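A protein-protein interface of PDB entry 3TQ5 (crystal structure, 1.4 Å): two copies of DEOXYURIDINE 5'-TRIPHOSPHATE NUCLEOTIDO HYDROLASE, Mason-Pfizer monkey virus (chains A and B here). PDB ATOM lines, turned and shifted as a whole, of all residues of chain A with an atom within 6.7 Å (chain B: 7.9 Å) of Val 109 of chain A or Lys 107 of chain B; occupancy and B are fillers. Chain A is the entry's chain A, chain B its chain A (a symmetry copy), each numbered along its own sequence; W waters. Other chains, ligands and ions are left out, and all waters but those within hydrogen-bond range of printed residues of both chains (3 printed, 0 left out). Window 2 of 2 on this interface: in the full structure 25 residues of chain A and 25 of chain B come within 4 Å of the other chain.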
ATOM      1  N   THR A  52      21.181 -38.776 -26.996  1.00  0.00           N
ATOM      2  CA  THR A  52      19.827 -38.260 -27.160  1.00  0.00           C
ATOM      3  C   THR A  52      19.220 -37.954 -25.799  1.00  0.00           C
ATOM      4  O   THR A  52      19.692 -38.435 -24.813  1.00  0.00           O
ATOM      5  CB  THR A  52      18.950 -39.280 -27.848  1.00  0.00           C
ATOM      6  OG1 THR A  52      18.936 -40.419 -27.026  1.00  0.00           O
ATOM      7  CG2 THR A  52      19.551 -39.750 -29.249  1.00  0.00           C
ATOM      8  N   PRO A  53      18.228 -37.095 -25.791  1.00  0.00           N
ATOM      9  CA  PRO A  53      17.674 -36.745 -24.452  1.00  0.00           C
ATOM     10  C   PRO A  53      17.177 -37.943 -23.641  1.00  0.00           C
ATOM     11  O   PRO A  53      17.479 -38.053 -22.432  1.00  0.00           O
ATOM     12  CB  PRO A  53      16.542 -35.799 -24.799  1.00  0.00           C
ATOM     13  CG  PRO A  53      17.000 -35.158 -26.161  1.00  0.00           C
ATOM     14  CD  PRO A  53      17.646 -36.325 -26.885  1.00  0.00           C
ATOM     15  N   THR A  83      27.617 -26.077 -23.887  1.00  0.00           N
ATOM     16  CA  THR A  83      26.298 -25.963 -23.283  1.00  0.00           C
ATOM     17  C   THR A  83      25.278 -25.255 -24.203  1.00  0.00           C
ATOM     18  O   THR A  83      24.114 -25.693 -24.324  1.00  0.00           O
ATOM     19  CB  THR A  83      26.453 -25.095 -21.999  1.00  0.00           C
ATOM     20  OG1 THR A  83      27.452 -25.673 -21.157  1.00  0.00           O
ATOM     21  CG2 THR A  83      25.099 -24.993 -21.225  1.00  0.00           C
ATOM     22  N   GLY A  86      23.647 -27.465 -26.661  1.00  0.00           N
ATOM     23  CA  GLY A  86      22.635 -28.420 -26.189  1.00  0.00           C
ATOM     24  C   GLY A  86      23.193 -29.616 -25.478  1.00  0.00           C
ATOM     25  O   GLY A  86      22.442 -30.576 -25.222  1.00  0.00           O
ATOM     26  N   LEU A  87      24.463 -29.558 -25.101  1.00  0.00           N
ATOM     27  CA  LEU A  87      25.025 -30.676 -24.342  1.00  0.00           C
ATOM     28  C   LEU A  87      25.322 -30.160 -22.967  1.00  0.00           C
ATOM     29  O   LEU A  87      26.161 -29.241 -22.808  1.00  0.00           O
ATOM     30  CB  LEU A  87      26.281 -31.220 -25.046  1.00  0.00           C
ATOM     31  CG  LEU A  87      27.004 -32.387 -24.368  1.00  0.00           C
ATOM     32  CD1 LEU A  87      26.129 -33.620 -24.386  1.00  0.00           C
ATOM     33  CD2 LEU A  87      28.296 -32.734 -25.079  1.00  0.00           C
ATOM     34  N   GLN A  88      24.647 -30.725 -21.966  1.00  0.00           N
ATOM     35  CA  GLN A  88      24.792 -30.279 -20.570  1.00  0.00           C
ATOM     36  C   GLN A  88      25.839 -31.168 -19.897  1.00  0.00           C
ATOM     37  O   GLN A  88      25.798 -32.413 -19.964  1.00  0.00           O
ATOM     38  CB  GLN A  88      23.507 -30.464 -19.816  1.00  0.00           C
ATOM     39  CG  GLN A  88      23.712 -30.287 -18.326  1.00  0.00           C
ATOM     40  CD  GLN A  88      22.397 -30.372 -17.607  1.00  0.00           C
ATOM     41  OE1 GLN A  88      21.393 -30.837 -18.162  1.00  0.00           O
ATOM     42  NE2 GLN A  88      22.373 -29.927 -16.386  1.00  0.00           N
ATOM     43  N   LYS A 107      24.653 -34.874 -20.792  1.00  0.00           N
ATOM     44  CA  LYS A 107      23.308 -35.226 -21.235  1.00  0.00           C
ATOM     45  C   LYS A 107      22.934 -34.320 -22.366  1.00  0.00           C
ATOM     46  O   LYS A 107      23.116 -33.120 -22.286  1.00  0.00           O
ATOM     47  CB  LYS A 107      22.279 -35.123 -20.104  1.00  0.00           C
ATOM     48  CG  LYS A 107      20.875 -35.628 -20.637  1.00  0.00           C
ATOM     49  CD  LYS A 107      19.728 -35.477 -19.715  1.00  0.00           C
ATOM     50  CE  LYS A 107      18.332 -35.659 -20.422  1.00  0.00           C
ATOM     51  NZ  LYS A 107      17.761 -34.436 -21.161  1.00  0.00           N
ATOM     52  N   ALA A 108      22.365 -34.861 -23.441  1.00  0.00           N
ATOM     53  CA  ALA A 108      21.755 -34.005 -24.476  1.00  0.00           C
ATOM     54  C   ALA A 108      20.453 -33.450 -23.924  1.00  0.00           C
ATOM     55  O   ALA A 108      19.571 -34.161 -23.454  1.00  0.00           O
ATOM     56  CB  ALA A 108      21.447 -34.874 -25.700  1.00  0.00           C
ATOM     57  N   VAL A 109      20.309 -32.121 -23.987  1.00  0.00           N
ATOM     58  CA  VAL A 109      19.219 -31.415 -23.315  1.00  0.00           C
ATOM     59  C   VAL A 109      17.862 -31.674 -24.017  1.00  0.00           C
ATOM     60  O   VAL A 109      16.889 -32.153 -23.393  1.00  0.00           O
ATOM     61  CB  VAL A 109      19.604 -29.900 -23.248  1.00  0.00           C
ATOM     62  CG1 VAL A 109      18.425 -29.012 -22.932  1.00  0.00           C
ATOM     63  CG2 VAL A 109      20.771 -29.692 -22.261  1.00  0.00           C
ATOM     64  N   ASN A 110      17.842 -31.317 -25.309  1.00  0.00           N
ATOM     65  CA  ASN A 110      16.608 -31.381 -26.085  1.00  0.00           C
ATOM     66  C   ASN A 110      16.681 -32.107 -27.422  1.00  0.00           C
ATOM     67  O   ASN A 110      15.632 -32.609 -27.921  1.00  0.00           O
ATOM     68  CB  ASN A 110      16.106 -29.942 -26.339  1.00  0.00           C
ATOM     69  CG  ASN A 110      15.185 -29.453 -25.265  1.00  0.00           C
ATOM     70  OD1 ASN A 110      15.037 -28.248 -25.061  1.00  0.00           O
ATOM     71  ND2 ASN A 110      14.541 -30.379 -24.573  1.00  0.00           N
ATOM     72  N   ASN A 111      17.877 -32.135 -28.002  1.00  0.00           N
ATOM     73  CA  ASN A 111      18.134 -32.572 -29.344  1.00  0.00           C
ATOM     74  C   ASN A 111      19.167 -33.660 -29.338  1.00  0.00           C
ATOM     75  O   ASN A 111      19.847 -33.837 -28.335  1.00  0.00           O
ATOM     76  CB  ASN A 111      18.742 -31.431 -30.154  1.00  0.00           C
ATOM     77  CG  ASN A 111      17.829 -30.225 -30.232  1.00  0.00           C
ATOM     78  OD1 ASN A 111      16.619 -30.365 -30.366  1.00  0.00           O
ATOM     79  ND2 ASN A 111      18.414 -29.029 -30.127  1.00  0.00           N
ATOM     80  N   VAL A 113      22.741 -34.900 -30.027  1.00  0.00           N
ATOM     81  CA  VAL A 113      24.107 -34.295 -30.027  1.00  0.00           C
ATOM     82  C   VAL A 113      25.128 -35.330 -30.431  1.00  0.00           C
ATOM     83  O   VAL A 113      25.084 -36.433 -29.920  1.00  0.00           O
ATOM     84  CB  VAL A 113      24.516 -33.869 -28.586  1.00  0.00           C
ATOM     85  CG1 VAL A 113      25.977 -33.370 -28.577  1.00  0.00           C
ATOM     86  CG2 VAL A 113      23.599 -32.816 -28.081  1.00  0.00           C
ATOM     87  N   LEU B  51      10.961 -17.963 -21.730  1.00  0.00           N
ATOM     88  CA  LEU B  51      11.690 -19.213 -22.061  1.00  0.00           C
ATOM     89  C   LEU B  51      10.744 -20.390 -21.937  1.00  0.00           C
ATOM     90  O   LEU B  51       9.972 -20.479 -20.985  1.00  0.00           O
ATOM     91  CB  LEU B  51      12.858 -19.484 -21.088  1.00  0.00           C
ATOM     92  CG  LEU B  51      13.860 -18.337 -20.972  1.00  0.00           C
ATOM     93  CD1 LEU B  51      14.874 -18.656 -19.846  1.00  0.00           C
ATOM     94  CD2 LEU B  51      14.527 -18.101 -22.312  1.00  0.00           C
ATOM     95  N   THR B  52      10.827 -21.302 -22.883  1.00  0.00           N
ATOM     96  CA  THR B  52      10.081 -22.552 -22.793  1.00  0.00           C
ATOM     97  C   THR B  52      11.040 -23.733 -22.831  1.00  0.00           C
ATOM     98  O   THR B  52      12.151 -23.585 -23.247  1.00  0.00           O
ATOM     99  CB  THR B  52       9.124 -22.686 -23.954  1.00  0.00           C
ATOM    100  OG1 THR B  52       9.904 -22.672 -25.122  1.00  0.00           O
ATOM    101  CG2 THR B  52       8.132 -21.441 -24.067  1.00  0.00           C
ATOM    102  N   PRO B  53      10.593 -24.857 -22.323  1.00  0.00           N
ATOM    103  CA  PRO B  53      11.552 -25.995 -22.303  1.00  0.00           C
ATOM    104  C   PRO B  53      12.119 -26.370 -23.673  1.00  0.00           C
ATOM    105  O   PRO B  53      13.344 -26.580 -23.812  1.00  0.00           O
ATOM    106  CB  PRO B  53      10.721 -27.120 -21.717  1.00  0.00           C
ATOM    107  CG  PRO B  53       9.661 -26.370 -20.828  1.00  0.00           C
ATOM    108  CD  PRO B  53       9.327 -25.144 -21.658  1.00  0.00           C
ATOM    109  N   GLU B  54      11.280 -26.346 -24.704  1.00  0.00           N
ATOM    110  CA  GLU B  54      11.773 -26.763 -26.011  1.00  0.00           C
ATOM    111  C   GLU B  54      12.779 -25.812 -26.593  1.00  0.00           C
ATOM    112  O   GLU B  54      13.474 -26.180 -27.542  1.00  0.00           O
ATOM    113  CB  GLU B  54      10.608 -27.018 -26.997  1.00  0.00           C
ATOM    114  CG  GLU B  54       9.890 -25.736 -27.431  1.00  0.00           C
ATOM    115  CD  GLU B  54       8.779 -25.338 -26.484  1.00  0.00           C
ATOM    116  OE1 GLU B  54       8.596 -25.969 -25.357  1.00  0.00           O
ATOM    117  OE2 GLU B  54       8.060 -24.382 -26.943  1.00  0.00           O
ATOM    118  N   MET B  55      12.909 -24.600 -26.052  1.00  0.00           N
ATOM    119  CA  MET B  55      13.943 -23.701 -26.536  1.00  0.00           C
ATOM    120  C   MET B  55      15.371 -24.105 -26.215  1.00  0.00           C
ATOM    121  O   MET B  55      16.327 -23.606 -26.834  1.00  0.00           O
ATOM    122  CB  MET B  55      13.727 -22.286 -26.004  1.00  0.00           C
ATOM    123  CG  MET B  55      12.664 -21.527 -26.793  1.00  0.00           C
ATOM    124  SD  MET B  55      12.147 -20.057 -25.833  1.00  0.00           S
ATOM    125  CE  MET B  55      13.497 -18.977 -26.157  1.00  0.00           C
ATOM    126  N   GLY B  56      15.526 -24.920 -25.202  1.00  0.00           N
ATOM    127  CA  GLY B  56      16.928 -25.234 -24.824  1.00  0.00           C
ATOM    128  C   GLY B  56      17.685 -24.038 -24.258  1.00  0.00           C
ATOM    129  O   GLY B  56      17.055 -23.029 -23.850  1.00  0.00           O
ATOM    130  N   PRO B  57      19.024 -24.177 -24.128  1.00  0.00           N
ATOM    131  CA  PRO B  57      19.777 -23.130 -23.454  1.00  0.00           C
ATOM    132  C   PRO B  57      19.746 -21.796 -24.152  1.00  0.00           C
ATOM    133  O   PRO B  57      19.903 -21.719 -25.369  1.00  0.00           O
ATOM    134  CB  PRO B  57      21.206 -23.694 -23.401  1.00  0.00           C
ATOM    135  CG  PRO B  57      20.980 -25.211 -23.401  1.00  0.00           C
ATOM    136  CD  PRO B  57      19.846 -25.377 -24.395  1.00  0.00           C
ATOM    137  N   GLN B  58      19.561 -20.753 -23.348  1.00  0.00           N
ATOM    138  CA  GLN B  58      19.510 -19.387 -23.859  1.00  0.00           C
ATOM    139  C   GLN B  58      20.496 -18.523 -23.108  1.00  0.00           C
ATOM    140  O   GLN B  58      20.579 -18.649 -21.877  1.00  0.00           O
ATOM    141  CB  GLN B  58      18.108 -18.807 -23.622  1.00  0.00           C
ATOM    142  CG  GLN B  58      17.021 -19.481 -24.407  1.00  0.00           C
ATOM    143  CD  GLN B  58      17.151 -19.347 -25.899  1.00  0.00           C
ATOM    144  OE1 GLN B  58      17.086 -18.234 -26.426  1.00  0.00           O
ATOM    145  NE2 GLN B  58      17.300 -20.482 -26.614  1.00  0.00           N
ATOM    146  N   ALA B  59      21.204 -17.632 -23.808  1.00  0.00           N
ATOM    147  CA  ALA B  59      22.212 -16.764 -23.127  1.00  0.00           C
ATOM    148  C   ALA B  59      21.566 -15.416 -22.861  1.00  0.00           C
ATOM    149  O   ALA B  59      21.261 -14.687 -23.828  1.00  0.00           O
ATOM    150  CB  ALA B  59      23.466 -16.620 -24.061  1.00  0.00           C
ATOM    151  N   LEU B  60      21.325 -15.096 -21.573  1.00  0.00           N
ATOM    152  CA  LEU B  60      20.640 -13.848 -21.182  1.00  0.00           C
ATOM    153  C   LEU B  60      21.666 -12.716 -21.020  1.00  0.00           C
ATOM    154  O   LEU B  60      22.683 -12.897 -20.352  1.00  0.00           O
ATOM    155  CB  LEU B  60      19.875 -14.039 -19.863  1.00  0.00           C
ATOM    156  CG  LEU B  60      18.909 -15.265 -19.931  1.00  0.00           C
ATOM    157  CD1 LEU B  60      18.248 -15.512 -18.585  1.00  0.00           C
ATOM    158  CD2 LEU B  60      17.848 -15.036 -21.035  1.00  0.00           C
ATOM    159  N   ILE B  82      15.082 -18.970  -7.692  1.00  0.00           N
ATOM    160  CA  ILE B  82      14.847 -18.969  -9.124  1.00  0.00           C
ATOM    161  C   ILE B  82      14.876 -20.424  -9.650  1.00  0.00           C
ATOM    162  O   ILE B  82      14.007 -20.854 -10.419  1.00  0.00           O
ATOM    163  CB  ILE B  82      15.895 -18.063  -9.770  1.00  0.00           C
ATOM    164  CG1 ILE B  82      15.750 -16.595  -9.249  1.00  0.00           C
ATOM    165  CG2 ILE B  82      15.867 -18.156 -11.285  1.00  0.00           C
ATOM    166  CD1 ILE B  82      14.702 -15.728  -9.976  1.00  0.00           C
ATOM    167  N   THR B  83      15.904 -21.199  -9.224  1.00  0.00           N
ATOM    168  CA  THR B  83      15.882 -22.607  -9.583  1.00  0.00           C
ATOM    169  C   THR B  83      14.589 -23.321  -9.130  1.00  0.00           C
ATOM    170  O   THR B  83      14.000 -24.122  -9.887  1.00  0.00           O
ATOM    171  CB  THR B  83      17.076 -23.288  -8.850  1.00  0.00           C
ATOM    172  OG1 THR B  83      18.285 -22.602  -9.179  1.00  0.00           O
ATOM    173  CG2 THR B  83      17.194 -24.795  -9.249  1.00  0.00           C
ATOM    174  N   GLY B  86      11.755 -22.978 -11.461  1.00  0.00           N
ATOM    175  CA  GLY B  86      11.786 -23.730 -12.724  1.00  0.00           C
ATOM    176  C   GLY B  86      12.712 -23.165 -13.760  1.00  0.00           C
ATOM    177  O   GLY B  86      12.659 -23.601 -14.926  1.00  0.00           O
ATOM    178  N   LEU B  87      13.592 -22.260 -13.356  1.00  0.00           N
ATOM    179  CA  LEU B  87      14.560 -21.736 -14.322  1.00  0.00           C
ATOM    180  C   LEU B  87      15.910 -22.221 -13.887  1.00  0.00           C
ATOM    181  O   LEU B  87      16.377 -21.868 -12.778  1.00  0.00           O
ATOM    182  CB  LEU B  87      14.480 -20.201 -14.378  1.00  0.00           C
ATOM    183  CG  LEU B  87      15.445 -19.491 -15.332  1.00  0.00           C
ATOM    184  CD1 LEU B  87      15.102 -19.833 -16.765  1.00  0.00           C
ATOM    185  CD2 LEU B  87      15.367 -17.985 -15.190  1.00  0.00           C
ATOM    186  N   GLN B  88      16.548 -23.029 -14.733  1.00  0.00           N
ATOM    187  CA  GLN B  88      17.854 -23.628 -14.413  1.00  0.00           C
ATOM    188  C   GLN B  88      18.943 -22.731 -15.005  1.00  0.00           C
ATOM    189  O   GLN B  88      18.910 -22.338 -16.188  1.00  0.00           O
ATOM    190  CB  GLN B  88      17.994 -24.976 -15.061  1.00  0.00           C
ATOM    191  CG  GLN B  88      19.422 -25.477 -14.988  1.00  0.00           C
ATOM    192  CD  GLN B  88      19.513 -26.867 -15.546  1.00  0.00           C
ATOM    193  OE1 GLN B  88      18.601 -27.341 -16.235  1.00  0.00           O
ATOM    194  NE2 GLN B  88      20.590 -27.538 -15.262  1.00  0.00           N
ATOM    195  N   VAL B  89      19.916 -22.333 -14.188  1.00  0.00           N
ATOM    196  CA  VAL B  89      21.111 -21.617 -14.703  1.00  0.00           C
ATOM    197  C   VAL B  89      22.241 -22.649 -14.757  1.00  0.00           C
ATOM    198  O   VAL B  89      22.526 -23.338 -13.770  1.00  0.00           O
ATOM    199  CB  VAL B  89      21.501 -20.451 -13.738  1.00  0.00           C
ATOM    200  CG1 VAL B  89      22.918 -19.910 -14.071  1.00  0.00           C
ATOM    201  CG2 VAL B  89      20.479 -19.376 -13.743  1.00  0.00           C
ATOM    202  N   TYR B  90      22.826 -22.831 -15.936  1.00  0.00           N
ATOM    203  CA  TYR B  90      23.931 -23.734 -16.103  1.00  0.00           C
ATOM    204  C   TYR B  90      25.171 -23.062 -15.540  1.00  0.00           C
ATOM    205  O   TYR B  90      25.437 -21.888 -15.920  1.00  0.00           O
ATOM    206  CB  TYR B  90      24.186 -24.069 -17.574  1.00  0.00           C
ATOM    207  CG  TYR B  90      23.028 -24.742 -18.245  1.00  0.00           C
ATOM    208  CD1 TYR B  90      22.815 -26.067 -18.019  1.00  0.00           C
ATOM    209  CD2 TYR B  90      22.138 -24.049 -19.068  1.00  0.00           C
ATOM    210  CE1 TYR B  90      21.730 -26.705 -18.618  1.00  0.00           C
ATOM    211  CE2 TYR B  90      21.021 -24.686 -19.675  1.00  0.00           C
ATOM    212  CZ  TYR B  90      20.865 -26.038 -19.431  1.00  0.00           C
ATOM    213  OH  TYR B  90      19.832 -26.769 -20.002  1.00  0.00           O
ATOM    214  N   ILE B 104      24.158 -15.073 -18.875  1.00  0.00           N
ATOM    215  CA  ILE B 104      23.660 -16.122 -18.018  1.00  0.00           C
ATOM    216  C   ILE B 104      23.100 -17.193 -18.959  1.00  0.00           C
ATOM    217  O   ILE B 104      22.303 -16.874 -19.844  1.00  0.00           O
ATOM    218  CB  ILE B 104      22.522 -15.607 -17.131  1.00  0.00           C
ATOM    219  CG1 ILE B 104      23.045 -14.501 -16.189  1.00  0.00           C
ATOM    220  CG2 ILE B 104      21.898 -16.704 -16.223  1.00  0.00           C
ATOM    221  CD1 ILE B 104      21.975 -13.612 -15.588  1.00  0.00           C
ATOM    222  N   MET B 105      23.561 -18.431 -18.810  1.00  0.00           N
ATOM    223  CA  MET B 105      23.034 -19.548 -19.665  1.00  0.00           C
ATOM    224  C   MET B 105      21.883 -20.170 -18.878  1.00  0.00           C
ATOM    225  O   MET B 105      22.121 -20.640 -17.782  1.00  0.00           O
ATOM    226  CB  MET B 105      24.111 -20.615 -19.883  1.00  0.00           C
ATOM    227  CG  MET B 105      25.318 -19.986 -20.633  1.00  0.00           C
ATOM    228  SD  MET B 105      26.503 -21.203 -21.103  1.00  0.00           S
ATOM    229  CE  MET B 105      27.107 -21.737 -19.463  1.00  0.00           C
ATOM    230  N   ALA B 106      20.680 -20.167 -19.447  1.00  0.00           N
ATOM    231  CA  ALA B 106      19.532 -20.589 -18.628  1.00  0.00           C
ATOM    232  C   ALA B 106      18.564 -21.373 -19.481  1.00  0.00           C
ATOM    233  O   ALA B 106      18.523 -21.267 -20.716  1.00  0.00           O
ATOM    234  CB  ALA B 106      18.861 -19.406 -18.058  1.00  0.00           C
ATOM    235  N   LYS B 107      17.767 -22.177 -18.781  1.00  0.00           N
ATOM    236  CA  LYS B 107      16.807 -23.025 -19.479  1.00  0.00           C
ATOM    237  C   LYS B 107      15.590 -23.165 -18.618  1.00  0.00           C
ATOM    238  O   LYS B 107      15.695 -23.429 -17.434  1.00  0.00           O
ATOM    239  CB  LYS B 107      17.385 -24.404 -19.815  1.00  0.00           C
ATOM    240  CG  LYS B 107      16.324 -25.214 -20.667  1.00  0.00           C
ATOM    241  CD  LYS B 107      16.663 -26.622 -20.972  1.00  0.00           C
ATOM    242  CE  LYS B 107      15.434 -27.458 -21.497  1.00  0.00           C
ATOM    243  NZ  LYS B 107      14.477 -28.031 -20.437  1.00  0.00           N
ATOM    244  N   ALA B 108      14.397 -23.029 -19.190  1.00  0.00           N
ATOM    245  CA  ALA B 108      13.169 -23.393 -18.458  1.00  0.00           C
ATOM    246  C   ALA B 108      13.091 -24.909 -18.390  1.00  0.00           C
ATOM    247  O   ALA B 108      13.167 -25.627 -19.382  1.00  0.00           O
ATOM    248  CB  ALA B 108      11.964 -22.868 -19.246  1.00  0.00           C
ATOM    249  N   VAL B 109      12.923 -25.433 -17.170  1.00  0.00           N
ATOM    250  CA  VAL B 109      13.039 -26.866 -16.907  1.00  0.00           C
ATOM    251  C   VAL B 109      11.836 -27.647 -17.492  1.00  0.00           C
ATOM    252  O   VAL B 109      12.002 -28.580 -18.309  1.00  0.00           O
ATOM    253  CB  VAL B 109      13.207 -27.054 -15.362  1.00  0.00           C
ATOM    254  CG1 VAL B 109      12.956 -28.474 -14.916  1.00  0.00           C
ATOM    255  CG2 VAL B 109      14.589 -26.537 -14.912  1.00  0.00           C
ATOM    256  N   ASN B 110      10.645 -27.242 -17.025  1.00  0.00           N
ATOM    257  CA  ASN B 110       9.420 -27.949 -17.382  1.00  0.00           C
ATOM    258  C   ASN B 110       8.271 -27.099 -17.906  1.00  0.00           C
ATOM    259  O   ASN B 110       7.391 -27.623 -18.650  1.00  0.00           O
ATOM    260  CB  ASN B 110       8.922 -28.734 -16.148  1.00  0.00           C
ATOM    261  CG  ASN B 110       9.482 -30.121 -16.080  1.00  0.00           C
ATOM    262  OD1 ASN B 110       9.557 -30.719 -15.006  1.00  0.00           O
ATOM    263  ND2 ASN B 110       9.868 -30.659 -17.226  1.00  0.00           N
ATOM    264  N   ASN B 111       8.258 -25.832 -17.506  1.00  0.00           N
ATOM    265  CA  ASN B 111       7.171 -24.915 -17.699  1.00  0.00           C
ATOM    266  C   ASN B 111       7.659 -23.688 -18.414  1.00  0.00           C
ATOM    267  O   ASN B 111       8.862 -23.470 -18.477  1.00  0.00           O
ATOM    268  CB  ASN B 111       6.656 -24.428 -16.349  1.00  0.00           C
ATOM    269  CG  ASN B 111       6.150 -25.560 -15.478  1.00  0.00           C
ATOM    270  OD1 ASN B 111       5.518 -26.490 -15.968  1.00  0.00           O
ATOM    271  ND2 ASN B 111       6.450 -25.491 -14.179  1.00  0.00           N
ATOM    272  N   VAL B 113       8.607 -19.962 -18.420  1.00  0.00           N
ATOM    273  CA  VAL B 113       9.167 -18.995 -17.429  1.00  0.00           C
ATOM    274  C   VAL B 113       9.277 -17.625 -18.054  1.00  0.00           C
ATOM    275  O   VAL B 113       9.761 -17.520 -19.164  1.00  0.00           O
ATOM    276  CB  VAL B 113      10.628 -19.382 -17.052  1.00  0.00           C
ATOM    277  CG1 VAL B 113      11.240 -18.302 -16.134  1.00  0.00           C
ATOM    278  CG2 VAL B 113      10.653 -20.709 -16.390  1.00  0.00           C
HETATM  279  O   HOH W   1      13.130 -29.819 -22.357  1.00  0.00           O
HETATM  280  O   HOH W   2      11.131 -29.711 -24.230  1.00  0.00           O
HETATM  281  O   HOH W   3      19.082 -28.820 -18.784  1.00  0.00           O
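The backbone NH (N) of Gly 56 of chain B sits at hydrogen-bond distance from the side-chain amide oxygen (OD1) of Asn 110 of chain A. OD1 of Asn 110 of chain A sits close to O of Pro 53 of chain B (2.7 Å). The side-chain amide nitrogen (NE2) of Gln 88 of chain A lies close to the side-chain amide nitrogen (NE2) of Gln 88 of chain B (3.2 Å).
The side-chain hydroxyl (OG1) of Thr 52 of chain B sits at hydrogen-bond distance from the side-chain carboxylate (OE2) of Glu 54 of chain B (3.1 Å). O of Gln 88 of chain B sits at hydrogen-bond distance from N of Lys 107 of chain B, 2.8 Å away. N of Val 109 of chain A lies within hydrogen-bond range of O of Gly 86 of chain A. N of Lys 107 of chain A sits at hydrogen-bond distance from O of Gln 88 of chain A (2.8 Å). The backbone carbonyl oxygen (O) of Val 109 of chain A is in hydrogen-bond range of the side-chain amino group (NZ) of Lys 107 of chain A (3.3 Å). The backbone carbonyl oxygen (O) of Val 109 of chain B is in hydrogen-bond range of the side-chain amino group (NZ) of Lys 107 of chain B.
O of Thr 83 of chain A touches CG of Pro 57 of chain B (3.3 Å). CG2 of Thr 83 of chain A touches CG of Tyr 90 of chain B, at 3.6 Å. Met 105 of chain B touches Thr 83 of chain A. CD of Gln 88 of chain A touches CE1 of Tyr 90 of chain B (3.9 Å). Val 109 of chain A touches Tyr 90 of chain B (CG2 to OH, 3.8 Å). Lys 107 of chain B touches Val 109 of chain A. OD1 of Asn 110 of chain A touches O of Glu 54 of chain B, 3.6 Å away. Asn 110 of chain A touches Lys 107 of chain B (OD1 to CE, 3.7 Å).
Printed residues of chain A within 4 Å of Lys 107 of chain B: Val 109 (3.6 Å) and Asn 110 (3.7 Å). Of the printed residues of chain A, Tyr 90 of chain B touches Thr 83, Gln 88 and Val 109. Of the printed residues of chain B, Gln 88 of chain A touches Gln 88 and Tyr 90. Of the printed residues of chain A, Pro 53 of chain B touches Asn 110. Printed residues of chain A within 4 Å of Glu 54 of chain B: Asn 110 (3.6 Å). Of the printed residues of chain A, Pro 57 of chain B touches Thr 83. Val 113 of chain B touches none of the printed residues of chain A. The nearest printed residue of chain B that does not touch Val 109 of chain A is Pro 57 of chain B (4.2 Å). The nearest printed residue of chain A that does not touch Lys 107 of chain B is Gln 88 of chain A (6.9 Å). The nearest printed residue of chain A that does not touch Pro 57 of chain B is Val 109 of chain A (4.2 Å).
Hydrophobic or aromatic side chains of chain B within 4 Å of the printed part of chain A: Pro 57, Tyr 90 and Met 105. Among the printed residues, no Asp or Glu carboxylate lies within 4 Å of a Lys or Arg side-chain nitrogen of the other chain.
Gln 88 of chain A touches its own counterpart, Gln 88 of chain B. Val 109 of chain A touches Lys 107 of chain B, but with the chains exchanged Lys 107 of chain A does not touch Val 109 of chain B (8.7 Å). Asn 110 of chain A touches Pro 53 of chain B, but with the chains exchanged Pro 53 of chain A does not touch Asn 110 of chain B (11.3 Å). Asn 110 of chain A touches Lys 107 of chain B, but with the chains exchanged Lys 107 of chain A does not touch Asn 110 of chain B (9.6 Å). Positions printed for both chains: 52, 53, 83, 86, 87, 88, 107, 108, 109, 110, 111 and 113.
Water W3 lies within hydrogen-bond range of the side-chain hydroxyl of Tyr 90 of chain B (2.5 Å), the side-chain amide oxygen of Gln 88 of chain B (3.0 Å) and the side-chain amide oxygen of Gln 88 of chain A (3.1 Å). Water W1 bridges ND2 of Asn 110 of chain A (2.7 Å) and NZ of Lys 107 of chain B (2.9 Å). Water W2 bridges N of Glu 54 of chain B (3.4 Å) and ND2 of Asn 110 of chain A (3.5 Å).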
